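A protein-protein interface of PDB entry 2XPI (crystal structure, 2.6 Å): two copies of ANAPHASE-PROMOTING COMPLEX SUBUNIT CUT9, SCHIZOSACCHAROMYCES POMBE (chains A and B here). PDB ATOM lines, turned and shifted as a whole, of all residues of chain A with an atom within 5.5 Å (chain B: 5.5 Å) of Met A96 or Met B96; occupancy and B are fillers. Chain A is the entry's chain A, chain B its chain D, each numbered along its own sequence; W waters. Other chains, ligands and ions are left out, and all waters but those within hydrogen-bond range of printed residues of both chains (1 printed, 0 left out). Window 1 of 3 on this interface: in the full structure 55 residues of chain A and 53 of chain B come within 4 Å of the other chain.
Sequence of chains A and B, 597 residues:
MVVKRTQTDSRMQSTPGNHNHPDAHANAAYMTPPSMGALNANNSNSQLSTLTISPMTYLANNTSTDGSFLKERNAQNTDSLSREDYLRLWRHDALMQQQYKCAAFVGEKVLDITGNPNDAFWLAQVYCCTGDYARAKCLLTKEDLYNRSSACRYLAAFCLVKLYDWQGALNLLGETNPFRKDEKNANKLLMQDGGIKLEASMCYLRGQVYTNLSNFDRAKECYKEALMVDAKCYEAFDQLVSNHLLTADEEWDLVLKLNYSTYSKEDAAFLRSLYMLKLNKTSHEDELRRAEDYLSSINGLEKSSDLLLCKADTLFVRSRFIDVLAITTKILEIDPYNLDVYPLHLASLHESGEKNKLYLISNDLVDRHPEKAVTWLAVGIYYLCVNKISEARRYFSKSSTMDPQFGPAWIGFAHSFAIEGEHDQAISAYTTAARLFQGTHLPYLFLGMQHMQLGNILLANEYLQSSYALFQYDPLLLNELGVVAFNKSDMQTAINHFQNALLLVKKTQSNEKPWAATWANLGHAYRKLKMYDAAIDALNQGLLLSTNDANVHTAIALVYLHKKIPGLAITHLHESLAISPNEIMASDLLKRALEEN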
ATOM      1  N   THR A  50      12.525  32.154 -10.856  1.00  0.00           N
ATOM      2  CA  THR A  50      11.796  31.590  -9.736  1.00  0.00           C
ATOM      3  C   THR A  50      11.423  32.650  -8.699  1.00  0.00           C
ATOM      4  O   THR A  50      10.456  32.489  -7.983  1.00  0.00           O
ATOM      5  CB  THR A  50      12.554  30.438  -9.080  1.00  0.00           C
ATOM      6  OG1 THR A  50      13.836  30.900  -8.629  1.00  0.00           O
ATOM      7  CG2 THR A  50      12.744  29.333 -10.093  1.00  0.00           C
ATOM      8  N   ARG A  91       6.975  25.209   3.921  1.00  0.00           N
ATOM      9  CA  ARG A  91       7.687  24.391   2.952  1.00  0.00           C
ATOM     10  C   ARG A  91       8.951  25.112   2.514  1.00  0.00           C
ATOM     11  O   ARG A  91      10.029  24.533   2.477  1.00  0.00           O
ATOM     12  CB  ARG A  91       6.808  24.133   1.745  1.00  0.00           C
ATOM     13  CG  ARG A  91       7.548  23.594   0.570  1.00  0.00           C
ATOM     14  CD  ARG A  91       6.694  23.768  -0.674  1.00  0.00           C
ATOM     15  NE  ARG A  91       6.538  25.174  -1.031  1.00  0.00           N
ATOM     16  CZ  ARG A  91       5.579  25.634  -1.823  1.00  0.00           C
ATOM     17  NH1 ARG A  91       4.699  24.786  -2.320  1.00  0.00           N
ATOM     18  NH2 ARG A  91       5.497  26.936  -2.107  1.00  0.00           N
ATOM     19  N   HIS A  92       8.832  26.398   2.220  1.00  0.00           N
ATOM     20  CA  HIS A  92       9.974  27.147   1.722  1.00  0.00           C
ATOM     21  C   HIS A  92      11.150  27.127   2.693  1.00  0.00           C
ATOM     22  O   HIS A  92      12.309  26.948   2.299  1.00  0.00           O
ATOM     23  CB  HIS A  92       9.578  28.583   1.450  1.00  0.00           C
ATOM     24  CG  HIS A  92      10.456  29.266   0.461  1.00  0.00           C
ATOM     25  ND1 HIS A  92      10.560  28.847  -0.850  1.00  0.00           N
ATOM     26  CD2 HIS A  92      11.254  30.352   0.576  1.00  0.00           C
ATOM     27  CE1 HIS A  92      11.389  29.643  -1.499  1.00  0.00           C
ATOM     28  NE2 HIS A  92      11.824  30.563  -0.655  1.00  0.00           N
ATOM     29  N   ASP A  93      10.853  27.338   3.964  1.00  0.00           N
ATOM     30  CA  ASP A  93      11.908  27.432   4.946  1.00  0.00           C
ATOM     31  C   ASP A  93      12.511  26.052   5.176  1.00  0.00           C
ATOM     32  O   ASP A  93      13.716  25.921   5.369  1.00  0.00           O
ATOM     33  CB  ASP A  93      11.390  28.048   6.235  1.00  0.00           C
ATOM     34  CG  ASP A  93      12.452  28.145   7.281  1.00  0.00           C
ATOM     35  OD1 ASP A  93      12.363  27.404   8.279  1.00  0.00           O
ATOM     36  OD2 ASP A  93      13.398  28.943   7.105  1.00  0.00           O
ATOM     37  N   ALA A  94      11.687  25.014   5.122  1.00  0.00           N
ATOM     38  CA  ALA A  94      12.210  23.649   5.245  1.00  0.00           C
ATOM     39  C   ALA A  94      13.298  23.379   4.195  1.00  0.00           C
ATOM     40  O   ALA A  94      14.387  22.936   4.522  1.00  0.00           O
ATOM     41  CB  ALA A  94      11.083  22.608   5.146  1.00  0.00           C
ATOM     42  N   LEU A  95      12.958  23.626   2.936  1.00  0.00           N
ATOM     43  CA  LEU A  95      13.856  23.540   1.809  1.00  0.00           C
ATOM     44  C   LEU A  95      15.158  24.249   2.155  1.00  0.00           C
ATOM     45  O   LEU A  95      16.232  23.654   2.178  1.00  0.00           O
ATOM     46  CB  LEU A  95      13.211  24.285   0.646  1.00  0.00           C
ATOM     47  CG  LEU A  95      13.075  23.635  -0.717  1.00  0.00           C
ATOM     48  CD1 LEU A  95      12.619  24.699  -1.740  1.00  0.00           C
ATOM     49  CD2 LEU A  95      14.384  23.005  -1.112  1.00  0.00           C
ATOM     50  N   MET A  96      15.031  25.536   2.442  1.00  0.00           N
ATOM     51  CA  MET A  96      16.155  26.395   2.715  1.00  0.00           C
ATOM     52  C   MET A  96      17.001  25.824   3.833  1.00  0.00           C
ATOM     53  O   MET A  96      18.203  26.019   3.853  1.00  0.00           O
ATOM     54  CB  MET A  96      15.636  27.770   3.113  1.00  0.00           C
ATOM     55  CG  MET A  96      16.066  28.926   2.224  1.00  0.00           C
ATOM     56  SD  MET A  96      15.332  29.040   0.592  1.00  0.00           S
ATOM     57  CE  MET A  96      16.253  27.779  -0.250  1.00  0.00           C
ATOM     58  N   GLN A  97      16.380  25.123   4.773  1.00  0.00           N
ATOM     59  CA  GLN A  97      17.109  24.599   5.916  1.00  0.00           C
ATOM     60  C   GLN A  97      17.505  23.146   5.707  1.00  0.00           C
ATOM     61  O   GLN A  97      18.036  22.502   6.623  1.00  0.00           O
ATOM     62  CB  GLN A  97      16.292  24.725   7.185  1.00  0.00           C
ATOM     63  CG  GLN A  97      16.043  26.141   7.637  1.00  0.00           C
ATOM     64  CD  GLN A  97      15.688  26.181   9.104  1.00  0.00           C
ATOM     65  OE1 GLN A  97      14.654  26.726   9.509  1.00  0.00           O
ATOM     66  NE2 GLN A  97      16.538  25.572   9.914  1.00  0.00           N
ATOM     67  N   GLN A  98      17.254  22.641   4.498  1.00  0.00           N
ATOM     68  CA  GLN A  98      17.662  21.289   4.122  1.00  0.00           C
ATOM     69  C   GLN A  98      17.055  20.259   5.040  1.00  0.00           C
ATOM     70  O   GLN A  98      17.652  19.221   5.320  1.00  0.00           O
ATOM     71  CB  GLN A  98      19.179  21.156   4.116  1.00  0.00           C
ATOM     72  CG  GLN A  98      19.846  22.207   3.270  1.00  0.00           C
ATOM     73  CD  GLN A  98      21.355  22.127   3.319  1.00  0.00           C
ATOM     74  OE1 GLN A  98      21.976  21.399   2.542  1.00  0.00           O
ATOM     75  NE2 GLN A  98      21.957  22.882   4.235  1.00  0.00           N
ATOM     76  N   PHE A 121       5.937  22.747  -8.770  1.00  0.00           N
ATOM     77  CA  PHE A 121       7.326  23.115  -8.971  1.00  0.00           C
ATOM     78  C   PHE A 121       8.140  22.975  -7.685  1.00  0.00           C
ATOM     79  O   PHE A 121       9.182  22.317  -7.650  1.00  0.00           O
ATOM     80  CB  PHE A 121       7.443  24.558  -9.456  1.00  0.00           C
ATOM     81  CG  PHE A 121       8.844  25.080  -9.418  1.00  0.00           C
ATOM     82  CD1 PHE A 121       9.763  24.713 -10.399  1.00  0.00           C
ATOM     83  CD2 PHE A 121       9.262  25.912  -8.392  1.00  0.00           C
ATOM     84  CE1 PHE A 121      11.082  25.185 -10.366  1.00  0.00           C
ATOM     85  CE2 PHE A 121      10.586  26.390  -8.344  1.00  0.00           C
ATOM     86  CZ  PHE A 121      11.495  26.019  -9.335  1.00  0.00           C
ATOM     87  N   TRP A 122       7.661  23.617  -6.630  1.00  0.00           N
ATOM     88  CA  TRP A 122       8.410  23.676  -5.385  1.00  0.00           C
ATOM     89  C   TRP A 122       8.531  22.308  -4.734  1.00  0.00           C
ATOM     90  O   TRP A 122       9.550  22.009  -4.092  1.00  0.00           O
ATOM     91  CB  TRP A 122       7.796  24.710  -4.443  1.00  0.00           C
ATOM     92  CG  TRP A 122       8.128  26.115  -4.861  1.00  0.00           C
ATOM     93  CD1 TRP A 122       7.258  27.077  -5.318  1.00  0.00           C
ATOM     94  CD2 TRP A 122       9.432  26.699  -4.906  1.00  0.00           C
ATOM     95  NE1 TRP A 122       7.945  28.227  -5.611  1.00  0.00           N
ATOM     96  CE2 TRP A 122       9.282  28.021  -5.368  1.00  0.00           C
ATOM     97  CE3 TRP A 122      10.717  26.232  -4.595  1.00  0.00           C
ATOM     98  CZ2 TRP A 122      10.374  28.891  -5.521  1.00  0.00           C
ATOM     99  CZ3 TRP A 122      11.807  27.104  -4.753  1.00  0.00           C
ATOM    100  CH2 TRP A 122      11.621  28.412  -5.211  1.00  0.00           C
ATOM    101  N   GLN A 125      11.157  20.555  -6.590  1.00  0.00           N
ATOM    102  CA  GLN A 125      12.450  21.063  -6.131  1.00  0.00           C
ATOM    103  C   GLN A 125      13.008  20.235  -4.998  1.00  0.00           C
ATOM    104  O   GLN A 125      14.200  19.889  -4.980  1.00  0.00           O
ATOM    105  CB  GLN A 125      12.304  22.484  -5.617  1.00  0.00           C
ATOM    106  CG  GLN A 125      12.635  23.546  -6.622  1.00  0.00           C
ATOM    107  CD  GLN A 125      14.113  23.648  -6.835  1.00  0.00           C
ATOM    108  OE1 GLN A 125      14.759  24.579  -6.358  1.00  0.00           O
ATOM    109  NE2 GLN A 125      14.671  22.674  -7.530  1.00  0.00           N
ATOM    110  N   THR B  50      15.034  31.171   8.449  1.00  0.00           N
ATOM    111  CA  THR B  50      15.777  31.527   7.250  1.00  0.00           C
ATOM    112  C   THR B  50      15.062  32.598   6.382  1.00  0.00           C
ATOM    113  O   THR B  50      15.695  33.328   5.615  1.00  0.00           O
ATOM    114  CB  THR B  50      16.017  30.226   6.453  1.00  0.00           C
ATOM    115  OG1 THR B  50      17.383  29.806   6.608  1.00  0.00           O
ATOM    116  CG2 THR B  50      15.643  30.387   5.006  1.00  0.00           C
ATOM    117  N   ARG B  91      22.054  35.846  -6.923  1.00  0.00           N
ATOM    118  CA  ARG B  91      22.551  34.635  -6.320  1.00  0.00           C
ATOM    119  C   ARG B  91      21.402  33.759  -5.817  1.00  0.00           C
ATOM    120  O   ARG B  91      21.484  32.541  -5.870  1.00  0.00           O
ATOM    121  CB  ARG B  91      23.523  34.933  -5.192  1.00  0.00           C
ATOM    122  CG  ARG B  91      22.950  34.594  -3.863  1.00  0.00           C
ATOM    123  CD  ARG B  91      23.977  34.183  -2.895  1.00  0.00           C
ATOM    124  NE  ARG B  91      24.348  35.299  -2.047  1.00  0.00           N
ATOM    125  CZ  ARG B  91      23.527  35.978  -1.249  1.00  0.00           C
ATOM    126  NH1 ARG B  91      22.241  35.683  -1.176  1.00  0.00           N
ATOM    127  NH2 ARG B  91      24.017  36.971  -0.521  1.00  0.00           N
ATOM    128  N   HIS B  92      20.324  34.371  -5.333  1.00  0.00           N
ATOM    129  CA  HIS B  92      19.233  33.605  -4.725  1.00  0.00           C
ATOM    130  C   HIS B  92      18.494  32.800  -5.782  1.00  0.00           C
ATOM    131  O   HIS B  92      18.187  31.623  -5.601  1.00  0.00           O
ATOM    132  CB  HIS B  92      18.247  34.518  -4.022  1.00  0.00           C
ATOM    133  CG  HIS B  92      17.344  33.783  -3.089  1.00  0.00           C
ATOM    134  ND1 HIS B  92      17.794  33.236  -1.906  1.00  0.00           N
ATOM    135  CD2 HIS B  92      16.041  33.442  -3.196  1.00  0.00           C
ATOM    136  CE1 HIS B  92      16.798  32.614  -1.307  1.00  0.00           C
ATOM    137  NE2 HIS B  92      15.724  32.722  -2.073  1.00  0.00           N
ATOM    138  N   ASP B  93      18.218  33.446  -6.901  1.00  0.00           N
ATOM    139  CA  ASP B  93      17.555  32.775  -7.986  1.00  0.00           C
ATOM    140  C   ASP B  93      18.443  31.695  -8.592  1.00  0.00           C
ATOM    141  O   ASP B  93      17.951  30.658  -9.029  1.00  0.00           O
ATOM    142  CB  ASP B  93      17.137  33.781  -9.039  1.00  0.00           C
ATOM    143  CG  ASP B  93      16.361  33.141 -10.173  1.00  0.00           C
ATOM    144  OD1 ASP B  93      15.370  32.396  -9.939  1.00  0.00           O
ATOM    145  OD2 ASP B  93      16.746  33.403 -11.320  1.00  0.00           O
ATOM    146  N   ALA B  94      19.751  31.931  -8.610  1.00  0.00           N
ATOM    147  CA  ALA B  94      20.704  30.949  -9.140  1.00  0.00           C
ATOM    148  C   ALA B  94      20.718  29.699  -8.274  1.00  0.00           C
ATOM    149  O   ALA B  94      20.840  28.589  -8.754  1.00  0.00           O
ATOM    150  CB  ALA B  94      22.115  31.555  -9.236  1.00  0.00           C
ATOM    151  N   LEU B  95      20.599  29.907  -6.976  1.00  0.00           N
ATOM    152  CA  LEU B  95      20.525  28.823  -6.024  1.00  0.00           C
ATOM    153  C   LEU B  95      19.237  28.028  -6.196  1.00  0.00           C
ATOM    154  O   LEU B  95      19.274  26.822  -6.261  1.00  0.00           O
ATOM    155  CB  LEU B  95      20.609  29.404  -4.633  1.00  0.00           C
ATOM    156  CG  LEU B  95      20.532  28.424  -3.491  1.00  0.00           C
ATOM    157  CD1 LEU B  95      21.674  27.453  -3.600  1.00  0.00           C
ATOM    158  CD2 LEU B  95      20.562  29.218  -2.168  1.00  0.00           C
ATOM    159  N   MET B  96      18.089  28.695  -6.279  1.00  0.00           N
ATOM    160  CA  MET B  96      16.833  27.975  -6.518  1.00  0.00           C
ATOM    161  C   MET B  96      16.813  27.250  -7.873  1.00  0.00           C
ATOM    162  O   MET B  96      16.075  26.284  -8.053  1.00  0.00           O
ATOM    163  CB  MET B  96      15.624  28.909  -6.445  1.00  0.00           C
ATOM    164  CG  MET B  96      15.575  29.846  -5.254  1.00  0.00           C
ATOM    165  SD  MET B  96      14.991  29.077  -3.756  1.00  0.00           S
ATOM    166  CE  MET B  96      16.248  27.826  -3.460  1.00  0.00           C
ATOM    167  N   GLN B  97      17.596  27.731  -8.835  1.00  0.00           N
ATOM    168  CA  GLN B  97      17.615  27.102 -10.152  1.00  0.00           C
ATOM    169  C   GLN B  97      18.762  26.104 -10.228  1.00  0.00           C
ATOM    170  O   GLN B  97      19.001  25.505 -11.279  1.00  0.00           O
ATOM    171  CB  GLN B  97      17.737  28.129 -11.275  1.00  0.00           C
ATOM    172  CG  GLN B  97      16.561  29.069 -11.422  1.00  0.00           C
ATOM    173  CD  GLN B  97      16.564  29.754 -12.770  1.00  0.00           C
ATOM    174  OE1 GLN B  97      16.849  29.128 -13.781  1.00  0.00           O
ATOM    175  NE2 GLN B  97      16.254  31.039 -12.795  1.00  0.00           N
ATOM    176  N   GLN B  98      19.452  25.926  -9.097  1.00  0.00           N
ATOM    177  CA  GLN B  98      20.554  24.971  -8.992  1.00  0.00           C
ATOM    178  C   GLN B  98      21.599  25.221 -10.059  1.00  0.00           C
ATOM    179  O   GLN B  98      22.078  24.289 -10.700  1.00  0.00           O
ATOM    180  CB  GLN B  98      20.046  23.536  -9.113  1.00  0.00           C
ATOM    181  CG  GLN B  98      18.840  23.199  -8.225  1.00  0.00           C
ATOM    182  CD  GLN B  98      18.316  21.809  -8.516  1.00  0.00           C
ATOM    183  OE1 GLN B  98      19.043  20.820  -8.379  1.00  0.00           O
ATOM    184  NE2 GLN B  98      17.070  21.726  -8.961  1.00  0.00           N
ATOM    185  N   PHE B 121      26.282  33.342   5.088  1.00  0.00           N
ATOM    186  CA  PHE B 121      25.360  32.217   5.220  1.00  0.00           C
ATOM    187  C   PHE B 121      24.912  31.660   3.870  1.00  0.00           C
ATOM    188  O   PHE B 121      24.973  30.461   3.624  1.00  0.00           O
ATOM    189  CB  PHE B 121      24.121  32.642   5.997  1.00  0.00           C
ATOM    190  CG  PHE B 121      23.021  31.650   5.938  1.00  0.00           C
ATOM    191  CD1 PHE B 121      23.032  30.540   6.765  1.00  0.00           C
ATOM    192  CD2 PHE B 121      21.972  31.813   5.038  1.00  0.00           C
ATOM    193  CE1 PHE B 121      22.004  29.604   6.702  1.00  0.00           C
ATOM    194  CE2 PHE B 121      20.937  30.889   4.959  1.00  0.00           C
ATOM    195  CZ  PHE B 121      20.943  29.781   5.794  1.00  0.00           C
ATOM    196  N   TRP B 122      24.433  32.539   3.002  1.00  0.00           N
ATOM    197  CA  TRP B 122      23.944  32.113   1.704  1.00  0.00           C
ATOM    198  C   TRP B 122      25.074  31.562   0.844  1.00  0.00           C
ATOM    199  O   TRP B 122      24.862  30.637   0.060  1.00  0.00           O
ATOM    200  CB  TRP B 122      23.201  33.255   1.012  1.00  0.00           C
ATOM    201  CG  TRP B 122      21.835  33.576   1.668  1.00  0.00           C
ATOM    202  CD1 TRP B 122      21.485  34.724   2.322  1.00  0.00           C
ATOM    203  CD2 TRP B 122      20.681  32.722   1.726  1.00  0.00           C
ATOM    204  NE1 TRP B 122      20.187  34.643   2.764  1.00  0.00           N
ATOM    205  CE2 TRP B 122      19.674  33.423   2.417  1.00  0.00           C
ATOM    206  CE3 TRP B 122      20.403  31.438   1.263  1.00  0.00           C
ATOM    207  CZ2 TRP B 122      18.403  32.874   2.660  1.00  0.00           C
ATOM    208  CZ3 TRP B 122      19.133  30.889   1.518  1.00  0.00           C
ATOM    209  CH2 TRP B 122      18.154  31.613   2.202  1.00  0.00           C
ATOM    210  N   GLN B 125      25.410  28.047   1.852  1.00  0.00           N
ATOM    211  CA  GLN B 125      24.307  27.291   1.275  1.00  0.00           C
ATOM    212  C   GLN B 125      24.744  26.667  -0.015  1.00  0.00           C
ATOM    213  O   GLN B 125      24.645  25.463  -0.193  1.00  0.00           O
ATOM    214  CB  GLN B 125      23.116  28.191   0.965  1.00  0.00           C
ATOM    215  CG  GLN B 125      22.201  28.427   2.114  1.00  0.00           C
ATOM    216  CD  GLN B 125      21.429  27.190   2.496  1.00  0.00           C
ATOM    217  OE1 GLN B 125      20.266  27.035   2.118  1.00  0.00           O
ATOM    218  NE2 GLN B 125      22.067  26.296   3.253  1.00  0.00           N
HETATM  219  O   HOH W   1      12.888  33.507  -1.041  1.00  0.00           O
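The side-chain amide oxygen (OE1) of Gln A125 lies close to the backbone carbonyl oxygen (O) of Met B96, at 2.7 Å.
The side-chain hydroxyl of Thr A50 lies within hydrogen-bond range of the side-chain carboxylate of Asp B93, 2.5 Å away.
NE2 of Gln A125 sits close to NE2 of Gln B98 (2.9 Å).
The side-chain carboxylate (OD2) of Asp A93 lies close to the backbone NH (N) of Thr B50.
O of Met A96 sits close to OE1 of Gln B125.
OD1 of Asp A93 lies close to OE1 of Gln A97, 2.7 Å away.
The side-chain carboxylate (OD2) of Asp B93 is in hydrogen-bond range of the side-chain amide nitrogen (NE2) of Gln B97, 2.8 Å away.
Met B96 touches Thr A50.
Met A96 touches Thr B50.
Met A96 touches Met B96.
Met A96 touches Trp B122.
Gln A98 touches Gln B125.
Trp A122 touches Met B96.
Of the printed residues of chain B, Asp A93 touches Thr B50 (3.0 Å).
Met A96 touches just these residues of chain B: Thr B50 (3.2 Å), Met B96 (3.2 Å), Trp B122 (3.4 Å) and Gln B125 (2.9 Å).
Phe A121 touches none of the printed residues of chain B.
Printed residues of chain B within 4 Å of Gln A125: Met B96 and Gln B98.
Printed residues of chain A within 4 Å of Thr B50: Asp A93 (3.0 Å) and Met A96 (3.2 Å).
Arg B91 touches none of the printed residues of chain A.
Of chain A, only Thr A50 (3.5 Å), Met A96 (3.2 Å), Trp A122 (3.7 Å) and Gln A125 (2.7 Å) come within 4 Å of Met B96.
Of the printed residues of chain A, Trp B122 touches Met A96.
The nearest residue of chain A that does not touch Met B96 is His A92 (4.3 Å).
Hydrophobic or aromatic side chains of chain B that line the printed part of chain A: Met B96 and Trp B122.
Of the 12 printed residues of chain A, 6 touch a printed residue of chain B.
Hydrophobic or aromatic side chains of chain A within 4 Å of the printed part of chain B: Met A96 and Trp A122.
Thr A50 touches Met B96, and with the chains exchanged Met A96 touches Thr B50.
Met B96 touches its own counterpart, Met A96.
Met A96 touches Trp B122, and with the chains exchanged Trp A122 touches Met B96.
Gln A98 touches Gln B125, and with the chains exchanged Gln A125 touches Gln B98.
Of the 11 pairs that touch across the chains among the printed residues, 11 have their exchanged pair printed and touching as well.
Water W1 bridges a ring nitrogen (NE2) of His B92 (3.1 Å) and a ring nitrogen (NE2) of His A92 (3.2 Å).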
